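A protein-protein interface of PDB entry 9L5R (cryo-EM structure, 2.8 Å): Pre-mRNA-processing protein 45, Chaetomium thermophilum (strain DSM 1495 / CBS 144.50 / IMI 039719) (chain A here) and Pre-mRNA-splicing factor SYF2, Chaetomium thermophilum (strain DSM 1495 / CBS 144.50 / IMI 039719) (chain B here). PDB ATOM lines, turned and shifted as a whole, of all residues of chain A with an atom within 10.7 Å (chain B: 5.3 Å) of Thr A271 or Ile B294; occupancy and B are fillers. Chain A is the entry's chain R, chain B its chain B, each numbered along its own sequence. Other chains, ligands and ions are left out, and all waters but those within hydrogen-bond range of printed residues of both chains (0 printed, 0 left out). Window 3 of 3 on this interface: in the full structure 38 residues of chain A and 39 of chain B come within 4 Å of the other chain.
Of the printed residues of chain B, Gly A269 touches Ile B294. Of the printed residues of chain B, Phe A270 touches Asn B295 and Asn B298. Of the printed residues of chain B, Thr A271 touches Thr B292, Ile B294, Asn B298 and Asn B302. Printed residues of chain B within 4 Å of Ile A272: Asn B302 (3.7 Å). Of the printed residues of chain B, Pro A273 touches Asn B302. Of chain A, only Thr A271 (2.9 Å) comes within 4 Å of Thr B292. Of chain A, only Gly A269 (3.2 Å) and Thr A271 (3.7 Å) come within 4 Å of Ile B294. Printed residues of chain A within 4 Å of Asn B302: Thr A271, Ile A272 and Pro A273. The nearest residue of chain B that does not touch Thr A271 is Tyr B293 (4.4 Å). The nearest printed residue of chain B that does not touch Ile A272 is Asn B298 (4.6 Å).
Of the 7 printed residues of chain B, 5 touch a printed residue of chain A. Hydrophobic or aromatic side chains of chain B that line the printed part of chain A: Ile B294. Along chain B the printed residues that touch a printed residue of chain A span positions 292 to 302. Of the 15 printed residues of chain A, 5 touch a printed residue of chain B. Hydrophobic or aromatic side chains of chain A that line the printed part of chain B: Phe A270, Ile A272 and Pro A273. Among the printed residues, no Asp or Glu carboxylate lies within 4 Å of a Lys or Arg side-chain nitrogen of the other chain.
N of Thr A271 is in hydrogen-bond range of OD1 of Asn B298 (2.9 Å). ND2 of Asn B302 is in hydrogen-bond range of O of Thr A271 (3.2 Å). O of Thr A271 sits close to O of Thr B292 (2.9 Å).
N of Asn B298 sits at hydrogen-bond distance from OD1 of Asn B295 (3.0 Å). O of Phe A270 sits at hydrogen-bond distance from ND2 of Asn A266 (2.6 Å). O of Thr B292 lies within hydrogen-bond range of ND2 of Asn B302, at 3.0 Å. ND2 of Asn B298 sits at hydrogen-bond distance from OD1 of Asn B302 (3.4 Å). The backbone NH of Ile B294 lies within hydrogen-bond range of the side-chain amide oxygen of Asn B298 (3.2 Å).
CD1 of Ile B294 touches O of Gly A269, at 3.2 Å. Phe A270 touches Asn B295. CD1 of Phe A270 touches CB of Asn B298, 3.6 Å away. CG2 of Ile B294 touches OG1 of Thr A271, 3.7 Å away. Asn B302 touches Ile A272 (OD1 to CD1, 3.7 Å). Pro A273 touches Asn B302.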
ATOM      1  N   VAL A 261      14.118  21.097  25.097  1.00  0.00           N
ATOM      2  CA  VAL A 261      14.204  22.549  25.070  1.00  0.00           C
ATOM      3  C   VAL A 261      15.073  22.967  26.240  1.00  0.00           C
ATOM      4  O   VAL A 261      14.702  22.749  27.398  1.00  0.00           O
ATOM      5  CB  VAL A 261      12.821  23.212  25.159  1.00  0.00           C
ATOM      6  CG1 VAL A 261      12.926  24.684  24.837  1.00  0.00           C
ATOM      7  CG2 VAL A 261      11.869  22.555  24.226  1.00  0.00           C
ATOM      8  N   SER A 262      16.224  23.555  25.951  1.00  0.00           N
ATOM      9  CA  SER A 262      17.095  24.046  27.005  1.00  0.00           C
ATOM     10  C   SER A 262      16.629  25.394  27.524  1.00  0.00           C
ATOM     11  O   SER A 262      16.118  26.223  26.779  1.00  0.00           O
ATOM     12  CB  SER A 262      18.529  24.175  26.509  1.00  0.00           C
ATOM     13  OG  SER A 262      19.375  24.594  27.549  1.00  0.00           O
ATOM     14  N   LYS A 265      20.631  26.994  26.457  1.00  0.00           N
ATOM     15  CA  LYS A 265      21.292  26.816  25.173  1.00  0.00           C
ATOM     16  C   LYS A 265      20.310  26.950  24.027  1.00  0.00           C
ATOM     17  O   LYS A 265      19.186  26.457  24.101  1.00  0.00           O
ATOM     18  CB  LYS A 265      21.963  25.446  25.092  1.00  0.00           C
ATOM     19  CG  LYS A 265      22.974  25.212  26.162  1.00  0.00           C
ATOM     20  CD  LYS A 265      24.145  26.109  25.955  1.00  0.00           C
ATOM     21  CE  LYS A 265      24.715  26.509  27.260  1.00  0.00           C
ATOM     22  NZ  LYS A 265      26.181  26.593  27.257  1.00  0.00           N
ATOM     23  N   ASN A 266      20.750  27.608  22.962  1.00  0.00           N
ATOM     24  CA  ASN A 266      20.009  27.655  21.703  1.00  0.00           C
ATOM     25  C   ASN A 266      21.002  27.761  20.551  1.00  0.00           C
ATOM     26  O   ASN A 266      21.179  28.825  19.966  1.00  0.00           O
ATOM     27  CB  ASN A 266      19.042  28.831  21.716  1.00  0.00           C
ATOM     28  CG  ASN A 266      18.058  28.799  20.607  1.00  0.00           C
ATOM     29  OD1 ASN A 266      17.864  27.791  19.954  1.00  0.00           O
ATOM     30  ND2 ASN A 266      17.381  29.906  20.412  1.00  0.00           N
ATOM     31  N   PRO A 267      21.696  26.663  20.220  1.00  0.00           N
ATOM     32  CA  PRO A 267      22.761  26.747  19.202  1.00  0.00           C
ATOM     33  C   PRO A 267      22.302  27.221  17.833  1.00  0.00           C
ATOM     34  O   PRO A 267      23.047  27.939  17.161  1.00  0.00           O
ATOM     35  CB  PRO A 267      23.298  25.315  19.146  1.00  0.00           C
ATOM     36  CG  PRO A 267      22.371  24.510  19.887  1.00  0.00           C
ATOM     37  CD  PRO A 267      21.717  25.358  20.883  1.00  0.00           C
ATOM     38  N   LYS A 268      21.090  26.894  17.416  1.00  0.00           N
ATOM     39  CA  LYS A 268      20.606  27.315  16.114  1.00  0.00           C
ATOM     40  C   LYS A 268      19.843  28.627  16.154  1.00  0.00           C
ATOM     41  O   LYS A 268      19.401  29.094  15.107  1.00  0.00           O
ATOM     42  CB  LYS A 268      19.734  26.224  15.511  1.00  0.00           C
ATOM     43  CG  LYS A 268      20.513  25.023  15.129  1.00  0.00           C
ATOM     44  CD  LYS A 268      19.633  23.975  14.534  1.00  0.00           C
ATOM     45  CE  LYS A 268      20.431  22.752  14.229  1.00  0.00           C
ATOM     46  NZ  LYS A 268      21.405  23.047  13.165  1.00  0.00           N
ATOM     47  N   GLY A 269      19.711  29.240  17.319  1.00  0.00           N
ATOM     48  CA  GLY A 269      18.990  30.482  17.431  1.00  0.00           C
ATOM     49  C   GLY A 269      17.501  30.388  17.216  1.00  0.00           C
ATOM     50  O   GLY A 269      16.898  31.371  16.802  1.00  0.00           O
ATOM     51  N   PHE A 270      16.893  29.239  17.495  1.00  0.00           N
ATOM     52  CA  PHE A 270      15.462  29.047  17.311  1.00  0.00           C
ATOM     53  C   PHE A 270      14.657  29.959  18.221  1.00  0.00           C
ATOM     54  O   PHE A 270      15.072  30.331  19.315  1.00  0.00           O
ATOM     55  CB  PHE A 270      15.031  27.618  17.631  1.00  0.00           C
ATOM     56  CG  PHE A 270      15.390  26.612  16.600  1.00  0.00           C
ATOM     57  CD1 PHE A 270      15.873  26.989  15.367  1.00  0.00           C
ATOM     58  CD2 PHE A 270      15.253  25.267  16.884  1.00  0.00           C
ATOM     59  CE1 PHE A 270      16.209  26.039  14.430  1.00  0.00           C
ATOM     60  CE2 PHE A 270      15.581  24.321  15.961  1.00  0.00           C
ATOM     61  CZ  PHE A 270      16.064  24.705  14.726  1.00  0.00           C
ATOM     62  N   THR A 271      13.485  30.295  17.755  1.00  0.00           N
ATOM     63  CA  THR A 271      12.479  30.966  18.555  1.00  0.00           C
ATOM     64  C   THR A 271      11.483  29.916  19.030  1.00  0.00           C
ATOM     65  O   THR A 271      10.735  29.354  18.232  1.00  0.00           O
ATOM     66  CB  THR A 271      11.835  32.071  17.727  1.00  0.00           C
ATOM     67  OG1 THR A 271      12.779  33.132  17.560  1.00  0.00           O
ATOM     68  CG2 THR A 271      10.688  32.612  18.396  1.00  0.00           C
ATOM     69  N   ILE A 272      11.510  29.621  20.318  1.00  0.00           N
ATOM     70  CA  ILE A 272      10.696  28.564  20.911  1.00  0.00           C
ATOM     71  C   ILE A 272       9.478  29.208  21.558  1.00  0.00           C
ATOM     72  O   ILE A 272       9.626  30.237  22.222  1.00  0.00           O
ATOM     73  CB  ILE A 272      11.516  27.754  21.928  1.00  0.00           C
ATOM     74  CG1 ILE A 272      12.758  27.169  21.258  1.00  0.00           C
ATOM     75  CG2 ILE A 272      10.694  26.676  22.583  1.00  0.00           C
ATOM     76  CD1 ILE A 272      12.463  26.239  20.146  1.00  0.00           C
ATOM     77  N   PRO A 273       8.271  28.669  21.383  1.00  0.00           N
ATOM     78  CA  PRO A 273       7.105  29.230  22.072  1.00  0.00           C
ATOM     79  C   PRO A 273       7.247  29.115  23.580  1.00  0.00           C
ATOM     80  O   PRO A 273       7.879  28.196  24.094  1.00  0.00           O
ATOM     81  CB  PRO A 273       5.947  28.383  21.552  1.00  0.00           C
ATOM     82  CG  PRO A 273       6.434  27.823  20.291  1.00  0.00           C
ATOM     83  CD  PRO A 273       7.882  27.589  20.466  1.00  0.00           C
ATOM     84  N   LEU A 274       6.671  30.081  24.288  1.00  0.00           N
ATOM     85  CA  LEU A 274       6.994  30.232  25.700  1.00  0.00           C
ATOM     86  C   LEU A 274       6.412  29.113  26.553  1.00  0.00           C
ATOM     87  O   LEU A 274       7.001  28.753  27.576  1.00  0.00           O
ATOM     88  CB  LEU A 274       6.534  31.603  26.187  1.00  0.00           C
ATOM     89  CG  LEU A 274       7.205  32.817  25.556  1.00  0.00           C
ATOM     90  CD1 LEU A 274       6.892  34.081  26.298  1.00  0.00           C
ATOM     91  CD2 LEU A 274       8.662  32.601  25.543  1.00  0.00           C
ATOM     92  N   ASP A 275       5.282  28.538  26.145  1.00  0.00           N
ATOM     93  CA  ASP A 275       4.767  27.358  26.830  1.00  0.00           C
ATOM     94  C   ASP A 275       5.713  26.170  26.676  1.00  0.00           C
ATOM     95  O   ASP A 275       5.931  25.412  27.626  1.00  0.00           O
ATOM     96  CB  ASP A 275       3.371  27.028  26.313  1.00  0.00           C
ATOM     97  CG  ASP A 275       3.363  26.648  24.847  1.00  0.00           C
ATOM     98  OD1 ASP A 275       3.460  27.552  23.995  1.00  0.00           O
ATOM     99  OD2 ASP A 275       3.260  25.443  24.542  1.00  0.00           O
ATOM    100  N   LYS A 276       6.311  26.016  25.498  1.00  0.00           N
ATOM    101  CA  LYS A 276       7.300  24.969  25.301  1.00  0.00           C
ATOM    102  C   LYS A 276       8.566  25.253  26.086  1.00  0.00           C
ATOM    103  O   LYS A 276       9.219  24.324  26.566  1.00  0.00           O
ATOM    104  CB  LYS A 276       7.619  24.823  23.818  1.00  0.00           C
ATOM    105  CG  LYS A 276       6.433  24.489  22.958  1.00  0.00           C
ATOM    106  CD  LYS A 276       5.681  23.317  23.501  1.00  0.00           C
ATOM    107  CE  LYS A 276       4.616  22.887  22.546  1.00  0.00           C
ATOM    108  NZ  LYS A 276       3.558  23.905  22.404  1.00  0.00           N
ATOM    109  N   ARG A 277       8.911  26.524  26.237  1.00  0.00           N
ATOM    110  CA  ARG A 277      10.074  26.891  27.021  1.00  0.00           C
ATOM    111  C   ARG A 277       9.869  26.635  28.504  1.00  0.00           C
ATOM    112  O   ARG A 277      10.829  26.302  29.205  1.00  0.00           O
ATOM    113  CB  ARG A 277      10.421  28.348  26.777  1.00  0.00           C
ATOM    114  CG  ARG A 277      11.374  28.520  25.654  1.00  0.00           C
ATOM    115  CD  ARG A 277      12.180  29.776  25.755  1.00  0.00           C
ATOM    116  NE  ARG A 277      12.967  29.947  24.547  1.00  0.00           N
ATOM    117  CZ  ARG A 277      14.102  29.321  24.296  1.00  0.00           C
ATOM    118  NH1 ARG A 277      14.653  28.518  25.181  1.00  0.00           N
ATOM    119  NH2 ARG A 277      14.692  29.498  23.125  1.00  0.00           N
ATOM    120  N   THR B 292       5.544  31.297  14.872  1.00  0.00           N
ATOM    121  CA  THR B 292       6.303  31.152  16.107  1.00  0.00           C
ATOM    122  C   THR B 292       7.764  30.839  15.840  1.00  0.00           C
ATOM    123  O   THR B 292       8.509  30.561  16.779  1.00  0.00           O
ATOM    124  CB  THR B 292       5.698  30.051  16.982  1.00  0.00           C
ATOM    125  OG1 THR B 292       5.473  28.884  16.191  1.00  0.00           O
ATOM    126  CG2 THR B 292       4.387  30.493  17.570  1.00  0.00           C
ATOM    127  N   TYR B 293       8.188  30.884  14.586  1.00  0.00           N
ATOM    128  CA  TYR B 293       9.461  30.364  14.125  1.00  0.00           C
ATOM    129  C   TYR B 293      10.163  31.453  13.332  1.00  0.00           C
ATOM    130  O   TYR B 293       9.610  32.524  13.098  1.00  0.00           O
ATOM    131  CB  TYR B 293       9.252  29.113  13.267  1.00  0.00           C
ATOM    132  CG  TYR B 293       8.109  29.267  12.290  1.00  0.00           C
ATOM    133  CD1 TYR B 293       8.313  29.828  11.038  1.00  0.00           C
ATOM    134  CD2 TYR B 293       6.822  28.869  12.626  1.00  0.00           C
ATOM    135  CE1 TYR B 293       7.278  29.985  10.164  1.00  0.00           C
ATOM    136  CE2 TYR B 293       5.785  29.028  11.757  1.00  0.00           C
ATOM    137  CZ  TYR B 293       6.016  29.584  10.530  1.00  0.00           C
ATOM    138  OH  TYR B 293       4.975  29.733   9.658  1.00  0.00           O
ATOM    139  N   ILE B 294      11.398  31.191  12.921  1.00  0.00           N
ATOM    140  CA  ILE B 294      12.129  32.175  12.130  1.00  0.00           C
ATOM    141  C   ILE B 294      12.748  31.544  10.896  1.00  0.00           C
ATOM    142  O   ILE B 294      13.244  32.255  10.023  1.00  0.00           O
ATOM    143  CB  ILE B 294      13.211  32.883  12.960  1.00  0.00           C
ATOM    144  CG1 ILE B 294      14.089  31.844  13.626  1.00  0.00           C
ATOM    145  CG2 ILE B 294      12.598  33.856  13.959  1.00  0.00           C
ATOM    146  CD1 ILE B 294      15.147  32.418  14.343  1.00  0.00           C
ATOM    147  N   ASN B 295      12.759  30.221  10.816  1.00  0.00           N
ATOM    148  CA  ASN B 295      13.099  29.561   9.565  1.00  0.00           C
ATOM    149  C   ASN B 295      12.379  28.226   9.500  1.00  0.00           C
ATOM    150  O   ASN B 295      11.554  27.899  10.351  1.00  0.00           O
ATOM    151  CB  ASN B 295      14.615  29.404   9.361  1.00  0.00           C
ATOM    152  CG  ASN B 295      15.338  28.852  10.565  1.00  0.00           C
ATOM    153  OD1 ASN B 295      14.978  27.818  11.105  1.00  0.00           O
ATOM    154  ND2 ASN B 295      16.397  29.532  10.967  1.00  0.00           N
ATOM    155  N   GLU B 296      12.703  27.460   8.461  1.00  0.00           N
ATOM    156  CA  GLU B 296      11.989  26.224   8.173  1.00  0.00           C
ATOM    157  C   GLU B 296      12.338  25.115   9.158  1.00  0.00           C
ATOM    158  O   GLU B 296      11.458  24.356   9.574  1.00  0.00           O
ATOM    159  CB  GLU B 296      12.287  25.790   6.738  1.00  0.00           C
ATOM    160  CG  GLU B 296      11.519  24.573   6.195  1.00  0.00           C
ATOM    161  CD  GLU B 296      10.072  24.436   6.650  1.00  0.00           C
ATOM    162  OE1 GLU B 296       9.330  25.437   6.728  1.00  0.00           O
ATOM    163  OE2 GLU B 296       9.676  23.294   6.941  1.00  0.00           O
ATOM    164  N   ASN B 298      13.247  25.640  12.199  1.00  0.00           N
ATOM    165  CA  ASN B 298      12.571  26.077  13.410  1.00  0.00           C
ATOM    166  C   ASN B 298      11.086  25.750  13.345  1.00  0.00           C
ATOM    167  O   ASN B 298      10.489  25.349  14.343  1.00  0.00           O
ATOM    168  CB  ASN B 298      12.800  27.572  13.594  1.00  0.00           C
ATOM    169  CG  ASN B 298      12.335  28.092  14.928  1.00  0.00           C
ATOM    170  OD1 ASN B 298      12.457  29.257  15.264  1.00  0.00           O
ATOM    171  ND2 ASN B 298      11.779  27.204  15.698  1.00  0.00           N
ATOM    172  N   ASN B 302       9.252  23.352  15.950  1.00  0.00           N
ATOM    173  CA  ASN B 302       8.113  23.813  16.729  1.00  0.00           C
ATOM    174  C   ASN B 302       6.895  22.934  16.512  1.00  0.00           C
ATOM    175  O   ASN B 302       6.109  22.731  17.440  1.00  0.00           O
ATOM    176  CB  ASN B 302       7.787  25.260  16.379  1.00  0.00           C
ATOM    177  CG  ASN B 302       8.679  26.244  17.086  1.00  0.00           C
ATOM    178  OD1 ASN B 302       9.564  25.863  17.841  1.00  0.00           O
ATOM    179  ND2 ASN B 302       8.461  27.519  16.835  1.00  0.00           N
